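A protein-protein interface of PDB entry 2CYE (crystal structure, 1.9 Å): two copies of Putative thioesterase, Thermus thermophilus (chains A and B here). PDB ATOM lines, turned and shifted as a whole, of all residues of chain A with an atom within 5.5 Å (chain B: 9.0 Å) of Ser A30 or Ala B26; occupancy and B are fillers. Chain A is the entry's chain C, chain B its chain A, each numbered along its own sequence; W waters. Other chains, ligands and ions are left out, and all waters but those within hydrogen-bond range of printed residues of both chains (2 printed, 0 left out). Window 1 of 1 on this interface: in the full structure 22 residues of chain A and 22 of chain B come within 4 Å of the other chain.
The backbone carbonyl oxygen (O) of Asp B16 sits at hydrogen-bond distance from the backbone NH (N) of Asn B24 (2.9 Å). The backbone carbonyl oxygen of Asn B25 lies within hydrogen-bond range of the side-chain hydroxyl of Tyr B62, at 2.8 Å. The side-chain carboxylate (OD2) of Asp B18 lies close to the side-chain amide oxygen (OD1) of Asn B24 (2.8 Å). ND2 of Asn B24 sits close to N of Ala B26.
Among the printed residues, merely in contact across the chains: Ala A26 with Ala B26, Ala A26 with Ser B30, Ser A30 with Ala B26, Leu A29 with Asn B25, Leu A29 with Leu B29, Leu A29 with Ala B26, Ala A26 with Leu B29 and Leu A29 with Tyr B62.
Water W1 lies within hydrogen-bond range of the side-chain carboxylate (OE1) of Glu A33 (2.7 Å), the side-chain amide nitrogen (ND2) of Asn B24 (2.8 Å) and the side-chain hydroxyl (OG) of Ser A30 (2.9 Å). Water W2 lies within hydrogen-bond range of the side-chain amide nitrogen (ND2) of Asn B25 and the backbone carbonyl oxygen (O) of Leu A29.
Val A27 touches none of the printed residues of chain B. Of the printed residues of chain B, Leu A29 touches Asn B25, Ala B26, Leu B29 and Tyr B62. Of the printed residues of chain B, Ser A30 touches Ala B26 (3.5 Å). Of the printed residues of chain B, Glu A33 touches Asn B24 (2.7 Å) and Asn B25 (3.1 Å). Of the printed residues of chain A, Asn B24 touches Glu A33. Of the printed residues of chain A, Asn B25 touches Leu A29 and Glu A33. Of chain A, only Ala A26 (3.4 Å), Leu A29 (3.7 Å) and Ser A30 (3.5 Å) come within 4 Å of Ala B26. Printed residues of chain A within 4 Å of Ser B30: Ala A26 (3.5 Å). Glu B33 touches none of the printed residues of chain A. The nearest residue of chain B that does not touch Ser A30 is Asn B24 (4.7 Å). The nearest residue of chain A that does not touch Ala B26 is Val A27 (5.3 Å).
Of the 17 printed residues of chain B, 6 touch a printed residue of chain A. Hydrophobic or aromatic side chains of chain B within 4 Å of the printed part of chain A: Ala B26, Leu B29 and Tyr B62. Along chain B the printed residues that touch a printed residue of chain A span positions 24 to 62. Of the 9 printed residues of chain A, 4 touch a printed residue of chain B. Hydrophobic or aromatic side chains of chain A that line the printed part of chain B: Ala A26 and Leu A29.
Ala A26 touches its own counterpart, Ala B26. Ala A26 touches Leu B29, and with the chains exchanged Leu A29 touches Ala B26. Ala A26 touches Ser B30, and with the chains exchanged Ser A30 touches Ala B26. Leu B29 touches its own counterpart, Leu A29. 8 positions are printed for both chains.
The side-chain carboxylate of Glu A33 sits close to the side-chain amide oxygen of Asn B25 (3.1 Å). The side-chain amide oxygen (OD1) of Asn B24 sits close to the side-chain carboxylate (OE2) of Glu A33, at 2.7 Å.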
ATOM      1  N   ALA A  26       0.662  29.581  23.590  1.00  0.00           N
ATOM      2  CA  ALA A  26       1.341  28.394  24.097  1.00  0.00           C
ATOM      3  C   ALA A  26       1.630  28.502  25.587  1.00  0.00           C
ATOM      4  O   ALA A  26       1.548  27.514  26.310  1.00  0.00           O
ATOM      5  CB  ALA A  26       2.625  28.169  23.344  1.00  0.00           C
ATOM      6  N   VAL A  27       1.939  29.709  26.049  1.00  0.00           N
ATOM      7  CA  VAL A  27       2.271  29.902  27.454  1.00  0.00           C
ATOM      8  C   VAL A  27       1.104  29.565  28.374  1.00  0.00           C
ATOM      9  O   VAL A  27       1.304  29.140  29.513  1.00  0.00           O
ATOM     10  CB  VAL A  27       2.776  31.330  27.685  1.00  0.00           C
ATOM     11  CG1 VAL A  27       3.047  31.568  29.157  1.00  0.00           C
ATOM     12  CG2 VAL A  27       4.058  31.536  26.875  1.00  0.00           C
ATOM     13  N   PHE A  28      -0.117  29.733  27.874  1.00  0.00           N
ATOM     14  CA  PHE A  28      -1.310  29.398  28.649  1.00  0.00           C
ATOM     15  C   PHE A  28      -1.254  27.937  29.071  1.00  0.00           C
ATOM     16  O   PHE A  28      -1.711  27.574  30.157  1.00  0.00           O
ATOM     17  CB  PHE A  28      -2.575  29.570  27.811  1.00  0.00           C
ATOM     18  CG  PHE A  28      -3.142  30.947  27.825  1.00  0.00           C
ATOM     19  CD1 PHE A  28      -4.262  31.243  28.613  1.00  0.00           C
ATOM     20  CD2 PHE A  28      -2.618  31.929  26.999  1.00  0.00           C
ATOM     21  CE1 PHE A  28      -4.846  32.484  28.564  1.00  0.00           C
ATOM     22  CE2 PHE A  28      -3.197  33.190  26.944  1.00  0.00           C
ATOM     23  CZ  PHE A  28      -4.320  33.470  27.728  1.00  0.00           C
ATOM     24  N   LEU A  29      -0.724  27.092  28.192  1.00  0.00           N
ATOM     25  CA  LEU A  29      -0.646  25.675  28.510  1.00  0.00           C
ATOM     26  C   LEU A  29       0.383  25.406  29.605  1.00  0.00           C
ATOM     27  O   LEU A  29       0.255  24.440  30.370  1.00  0.00           O
ATOM     28  CB  LEU A  29      -0.338  24.853  27.246  1.00  0.00           C
ATOM     29  CG  LEU A  29      -1.563  24.538  26.377  1.00  0.00           C
ATOM     30  CD1 LEU A  29      -2.173  25.839  25.809  1.00  0.00           C
ATOM     31  CD2 LEU A  29      -1.150  23.611  25.247  1.00  0.00           C
ATOM     32  N   SER A  30       1.398  26.266  29.696  1.00  0.00           N
ATOM     33  CA  SER A  30       2.413  26.099  30.737  1.00  0.00           C
ATOM     34  C   SER A  30       1.827  26.511  32.093  1.00  0.00           C
ATOM     35  O   SER A  30       2.212  25.976  33.132  1.00  0.00           O
ATOM     36  CB  SER A  30       3.660  26.921  30.401  1.00  0.00           C
ATOM     37  OG  SER A  30       4.251  26.433  29.201  1.00  0.00           O
ATOM     38  N   TYR A  31       0.902  27.471  32.072  1.00  0.00           N
ATOM     39  CA  TYR A  31       0.212  27.926  33.285  1.00  0.00           C
ATOM     40  C   TYR A  31      -0.630  26.749  33.783  1.00  0.00           C
ATOM     41  O   TYR A  31      -0.601  26.390  34.961  1.00  0.00           O
ATOM     42  CB  TYR A  31      -0.757  29.076  32.980  1.00  0.00           C
ATOM     43  CG  TYR A  31      -0.141  30.429  32.685  1.00  0.00           C
ATOM     44  CD1 TYR A  31       1.244  30.611  32.637  1.00  0.00           C
ATOM     45  CD2 TYR A  31      -0.958  31.539  32.452  1.00  0.00           C
ATOM     46  CE1 TYR A  31       1.800  31.867  32.361  1.00  0.00           C
ATOM     47  CE2 TYR A  31      -0.417  32.794  32.178  1.00  0.00           C
ATOM     48  CZ  TYR A  31       0.963  32.949  32.134  1.00  0.00           C
ATOM     49  OH  TYR A  31       1.502  34.193  31.872  1.00  0.00           O
ATOM     50  N   MET A  32      -1.409  26.177  32.872  1.00  0.00           N
ATOM     51  CA  MET A  32      -2.270  25.037  33.193  1.00  0.00           C
ATOM     52  C   MET A  32      -1.419  23.882  33.714  1.00  0.00           C
ATOM     53  O   MET A  32      -1.763  23.221  34.695  1.00  0.00           O
ATOM     54  CB  MET A  32      -3.036  24.582  31.939  1.00  0.00           C
ATOM     55  CG  MET A  32      -3.993  25.616  31.358  1.00  0.00           C
ATOM     56  SD  MET A  32      -4.869  25.102  29.830  1.00  0.00           S
ATOM     57  CE  MET A  32      -6.109  26.367  29.757  1.00  0.00           C
ATOM     58  N   GLU A  33      -0.301  23.644  33.045  1.00  0.00           N
ATOM     59  CA  GLU A  33       0.612  22.568  33.421  1.00  0.00           C
ATOM     60  C   GLU A  33       1.115  22.675  34.855  1.00  0.00           C
ATOM     61  O   GLU A  33       1.281  21.659  35.523  1.00  0.00           O
ATOM     62  CB  GLU A  33       1.815  22.564  32.482  1.00  0.00           C
ATOM     63  CG  GLU A  33       2.868  21.521  32.793  1.00  0.00           C
ATOM     64  CD  GLU A  33       3.985  21.567  31.782  1.00  0.00           C
ATOM     65  OE1 GLU A  33       4.798  22.520  31.830  1.00  0.00           O
ATOM     66  OE2 GLU A  33       4.028  20.666  30.921  1.00  0.00           O
ATOM     67  N   LEU A  34       1.373  23.894  35.331  1.00  0.00           N
ATOM     68  CA  LEU A  34       1.879  24.027  36.691  1.00  0.00           C
ATOM     69  C   LEU A  34       0.873  23.460  37.686  1.00  0.00           C
ATOM     70  O   LEU A  34       1.244  22.755  38.624  1.00  0.00           O
ATOM     71  CB  LEU A  34       2.196  25.492  37.019  1.00  0.00           C
ATOM     72  CG  LEU A  34       2.616  25.762  38.472  1.00  0.00           C
ATOM     73  CD1 LEU A  34       3.841  24.901  38.824  1.00  0.00           C
ATOM     74  CD2 LEU A  34       2.922  27.257  38.663  1.00  0.00           C
ATOM     75  N   ARG B  15      16.018  23.041  25.738  1.00  0.00           N
ATOM     76  CA  ARG B  15      15.049  23.804  26.535  1.00  0.00           C
ATOM     77  C   ARG B  15      13.604  23.412  26.264  1.00  0.00           C
ATOM     78  O   ARG B  15      12.728  23.670  27.087  1.00  0.00           O
ATOM     79  CB  ARG B  15      15.224  25.312  26.288  1.00  0.00           C
ATOM     80  CG  ARG B  15      14.342  26.234  27.159  1.00  0.00           C
ATOM     81  CD  ARG B  15      14.884  26.411  28.597  1.00  0.00           C
ATOM     82  NE  ARG B  15      14.518  25.303  29.486  1.00  0.00           N
ATOM     83  CZ  ARG B  15      13.332  25.169  30.067  1.00  0.00           C
ATOM     84  NH1 ARG B  15      13.093  24.124  30.844  1.00  0.00           N
ATOM     85  NH2 ARG B  15      12.387  26.088  29.891  1.00  0.00           N
ATOM     86  N   ASP B  16      13.352  22.795  25.113  1.00  0.00           N
ATOM     87  CA  ASP B  16      11.995  22.382  24.763  1.00  0.00           C
ATOM     88  C   ASP B  16      11.547  21.120  25.492  1.00  0.00           C
ATOM     89  O   ASP B  16      10.360  20.824  25.542  1.00  0.00           O
ATOM     90  CB  ASP B  16      11.894  22.065  23.269  1.00  0.00           C
ATOM     91  CG  ASP B  16      12.171  23.252  22.395  1.00  0.00           C
ATOM     92  OD1 ASP B  16      12.180  24.390  22.911  1.00  0.00           O
ATOM     93  OD2 ASP B  16      12.361  23.043  21.179  1.00  0.00           O
ATOM     94  N   ASP B  18      10.801  17.936  28.254  1.00  0.00           N
ATOM     95  CA  ASP B  18      10.267  17.573  29.558  1.00  0.00           C
ATOM     96  C   ASP B  18      11.410  16.733  30.134  1.00  0.00           C
ATOM     97  O   ASP B  18      12.307  16.332  29.396  1.00  0.00           O
ATOM     98  CB  ASP B  18       9.002  16.722  29.397  1.00  0.00           C
ATOM     99  CG  ASP B  18       7.769  17.566  29.145  1.00  0.00           C
ATOM    100  OD1 ASP B  18       6.848  17.082  28.489  1.00  0.00           O
ATOM    101  OD2 ASP B  18       7.726  18.729  29.608  1.00  0.00           O
ATOM    102  N   HIS B  22      11.533  14.332  25.966  1.00  0.00           N
ATOM    103  CA  HIS B  22      10.694  14.533  24.788  1.00  0.00           C
ATOM    104  C   HIS B  22      10.140  15.962  24.869  1.00  0.00           C
ATOM    105  O   HIS B  22      10.092  16.554  25.952  1.00  0.00           O
ATOM    106  CB  HIS B  22       9.561  13.505  24.734  1.00  0.00           C
ATOM    107  CG  HIS B  22       8.689  13.504  25.945  1.00  0.00           C
ATOM    108  ND1 HIS B  22       8.695  12.476  26.868  1.00  0.00           N
ATOM    109  CD2 HIS B  22       7.792  14.413  26.401  1.00  0.00           C
ATOM    110  CE1 HIS B  22       7.839  12.755  27.838  1.00  0.00           C
ATOM    111  NE2 HIS B  22       7.282  13.920  27.577  1.00  0.00           N
ATOM    112  N   VAL B  23       9.723  16.513  23.736  1.00  0.00           N
ATOM    113  CA  VAL B  23       9.223  17.884  23.700  1.00  0.00           C
ATOM    114  C   VAL B  23       7.971  18.118  24.540  1.00  0.00           C
ATOM    115  O   VAL B  23       7.025  17.329  24.503  1.00  0.00           O
ATOM    116  CB  VAL B  23       8.978  18.337  22.242  1.00  0.00           C
ATOM    117  CG1 VAL B  23       8.307  19.720  22.214  1.00  0.00           C
ATOM    118  CG2 VAL B  23      10.333  18.406  21.498  1.00  0.00           C
ATOM    119  N   ASN B  24       7.988  19.215  25.297  1.00  0.00           N
ATOM    120  CA  ASN B  24       6.885  19.597  26.172  1.00  0.00           C
ATOM    121  C   ASN B  24       5.624  19.965  25.373  1.00  0.00           C
ATOM    122  O   ASN B  24       5.712  20.595  24.324  1.00  0.00           O
ATOM    123  CB  ASN B  24       7.300  20.787  27.039  1.00  0.00           C
ATOM    124  CG  ASN B  24       6.167  21.275  27.916  1.00  0.00           C
ATOM    125  OD1 ASN B  24       5.902  20.716  28.985  1.00  0.00           O
ATOM    126  ND2 ASN B  24       5.469  22.299  27.451  1.00  0.00           N
ATOM    127  N   ASN B  25       4.461  19.587  25.894  1.00  0.00           N
ATOM    128  CA  ASN B  25       3.187  19.835  25.218  1.00  0.00           C
ATOM    129  C   ASN B  25       2.929  21.268  24.746  1.00  0.00           C
ATOM    130  O   ASN B  25       2.368  21.477  23.673  1.00  0.00           O
ATOM    131  CB  ASN B  25       2.020  19.381  26.107  1.00  0.00           C
ATOM    132  CG  ASN B  25       1.735  20.344  27.252  1.00  0.00           C
ATOM    133  OD1 ASN B  25       2.413  20.338  28.284  1.00  0.00           O
ATOM    134  ND2 ASN B  25       0.727  21.177  27.073  1.00  0.00           N
ATOM    135  N   ALA B  26       3.334  22.258  25.533  1.00  0.00           N
ATOM    136  CA  ALA B  26       3.090  23.646  25.144  1.00  0.00           C
ATOM    137  C   ALA B  26       4.021  24.089  24.020  1.00  0.00           C
ATOM    138  O   ALA B  26       3.644  24.888  23.155  1.00  0.00           O
ATOM    139  CB  ALA B  26       3.246  24.575  26.363  1.00  0.00           C
ATOM    140  N   VAL B  27       5.238  23.559  24.023  1.00  0.00           N
ATOM    141  CA  VAL B  27       6.195  23.942  23.004  1.00  0.00           C
ATOM    142  C   VAL B  27       5.707  23.548  21.606  1.00  0.00           C
ATOM    143  O   VAL B  27       6.072  24.187  20.629  1.00  0.00           O
ATOM    144  CB  VAL B  27       7.590  23.338  23.296  1.00  0.00           C
ATOM    145  CG1 VAL B  27       8.551  23.670  22.166  1.00  0.00           C
ATOM    146  CG2 VAL B  27       8.125  23.894  24.617  1.00  0.00           C
ATOM    147  N   PHE B  28       4.894  22.495  21.507  1.00  0.00           N
ATOM    148  CA  PHE B  28       4.353  22.099  20.205  1.00  0.00           C
ATOM    149  C   PHE B  28       3.566  23.260  19.591  1.00  0.00           C
ATOM    150  O   PHE B  28       3.583  23.463  18.373  1.00  0.00           O
ATOM    151  CB  PHE B  28       3.406  20.912  20.337  1.00  0.00           C
ATOM    152  CG  PHE B  28       4.092  19.577  20.419  1.00  0.00           C
ATOM    153  CD1 PHE B  28       4.699  19.160  21.595  1.00  0.00           C
ATOM    154  CD2 PHE B  28       4.081  18.713  19.328  1.00  0.00           C
ATOM    155  CE1 PHE B  28       5.279  17.902  21.692  1.00  0.00           C
ATOM    156  CE2 PHE B  28       4.656  17.455  19.410  1.00  0.00           C
ATOM    157  CZ  PHE B  28       5.257  17.044  20.598  1.00  0.00           C
ATOM    158  N   LEU B  29       2.851  24.007  20.430  1.00  0.00           N
ATOM    159  CA  LEU B  29       2.065  25.138  19.925  1.00  0.00           C
ATOM    160  C   LEU B  29       2.977  26.244  19.391  1.00  0.00           C
ATOM    161  O   LEU B  29       2.597  26.993  18.484  1.00  0.00           O
ATOM    162  CB  LEU B  29       1.137  25.698  21.019  1.00  0.00           C
ATOM    163  CG  LEU B  29      -0.199  24.961  21.213  1.00  0.00           C
ATOM    164  CD1 LEU B  29       0.055  23.523  21.678  1.00  0.00           C
ATOM    165  CD2 LEU B  29      -1.066  25.716  22.216  1.00  0.00           C
ATOM    166  N   SER B  30       4.179  26.345  19.948  1.00  0.00           N
ATOM    167  CA  SER B  30       5.135  27.344  19.489  1.00  0.00           C
ATOM    168  C   SER B  30       5.710  26.913  18.133  1.00  0.00           C
ATOM    169  O   SER B  30       6.047  27.758  17.296  1.00  0.00           O
ATOM    170  CB  SER B  30       6.241  27.528  20.531  1.00  0.00           C
ATOM    171  OG  SER B  30       5.709  28.115  21.712  1.00  0.00           O
ATOM    172  N   TYR B  31       5.819  25.604  17.913  1.00  0.00           N
ATOM    173  CA  TYR B  31       6.295  25.092  16.626  1.00  0.00           C
ATOM    174  C   TYR B  31       5.211  25.416  15.597  1.00  0.00           C
ATOM    175  O   TYR B  31       5.494  25.883  14.494  1.00  0.00           O
ATOM    176  CB  TYR B  31       6.469  23.563  16.650  1.00  0.00           C
ATOM    177  CG  TYR B  31       7.626  23.017  17.462  1.00  0.00           C
ATOM    178  CD1 TYR B  31       8.507  23.856  18.144  1.00  0.00           C
ATOM    179  CD2 TYR B  31       7.827  21.641  17.555  1.00  0.00           C
ATOM    180  CE1 TYR B  31       9.559  23.332  18.904  1.00  0.00           C
ATOM    181  CE2 TYR B  31       8.874  21.106  18.308  1.00  0.00           C
ATOM    182  CZ  TYR B  31       9.735  21.952  18.979  1.00  0.00           C
ATOM    183  OH  TYR B  31      10.772  21.413  19.722  1.00  0.00           O
ATOM    184  N   MET B  32       3.961  25.142  15.967  1.00  0.00           N
ATOM    185  CA  MET B  32       2.825  25.386  15.082  1.00  0.00           C
ATOM    186  C   MET B  32       2.721  26.866  14.745  1.00  0.00           C
ATOM    187  O   MET B  32       2.411  27.246  13.613  1.00  0.00           O
ATOM    188  CB  MET B  32       1.520  24.913  15.747  1.00  0.00           C
ATOM    189  CG  MET B  32       1.415  23.397  15.900  1.00  0.00           C
ATOM    190  SD  MET B  32      -0.025  22.819  16.813  1.00  0.00           S
ATOM    191  CE  MET B  32       0.249  21.060  16.734  1.00  0.00           C
ATOM    192  N   GLU B  33       2.995  27.697  15.739  1.00  0.00           N
ATOM    193  CA  GLU B  33       2.938  29.141  15.581  1.00  0.00           C
ATOM    194  C   GLU B  33       3.933  29.674  14.552  1.00  0.00           C
ATOM    195  O   GLU B  33       3.609  30.588  13.786  1.00  0.00           O
ATOM    196  CB  GLU B  33       3.201  29.781  16.930  1.00  0.00           C
ATOM    197  CG  GLU B  33       3.259  31.285  16.946  1.00  0.00           C
ATOM    198  CD  GLU B  33       3.416  31.777  18.358  1.00  0.00           C
ATOM    199  OE1 GLU B  33       4.530  31.621  18.924  1.00  0.00           O
ATOM    200  OE2 GLU B  33       2.416  32.286  18.904  1.00  0.00           O
ATOM    201  N   VAL B  60      -5.163  20.253  20.040  1.00  0.00           N
ATOM    202  CA  VAL B  60      -3.965  19.551  19.617  1.00  0.00           C
ATOM    203  C   VAL B  60      -3.943  18.091  20.022  1.00  0.00           C
ATOM    204  O   VAL B  60      -4.177  17.762  21.179  1.00  0.00           O
ATOM    205  CB  VAL B  60      -2.706  20.220  20.196  1.00  0.00           C
ATOM    206  CG1 VAL B  60      -1.477  19.443  19.785  1.00  0.00           C
ATOM    207  CG2 VAL B  60      -2.616  21.673  19.723  1.00  0.00           C
ATOM    208  N   TYR B  62      -1.482  14.961  20.231  1.00  0.00           N
ATOM    209  CA  TYR B  62      -0.066  14.606  20.301  1.00  0.00           C
ATOM    210  C   TYR B  62       0.006  13.132  19.915  1.00  0.00           C
ATOM    211  O   TYR B  62      -0.384  12.253  20.684  1.00  0.00           O
ATOM    212  CB  TYR B  62       0.437  14.848  21.724  1.00  0.00           C
ATOM    213  CG  TYR B  62       0.287  16.292  22.165  1.00  0.00           C
ATOM    214  CD1 TYR B  62       1.309  17.224  21.946  1.00  0.00           C
ATOM    215  CD2 TYR B  62      -0.885  16.733  22.773  1.00  0.00           C
ATOM    216  CE1 TYR B  62       1.160  18.562  22.325  1.00  0.00           C
ATOM    217  CE2 TYR B  62      -1.044  18.059  23.151  1.00  0.00           C
ATOM    218  CZ  TYR B  62      -0.018  18.972  22.926  1.00  0.00           C
ATOM    219  OH  TYR B  62      -0.179  20.288  23.315  1.00  0.00           O
HETATM  220  O   HOH W   1       4.154  23.598  29.491  1.00  0.00           O
HETATM  221  O   HOH W   2      -0.270  21.753  29.650  1.00  0.00           O
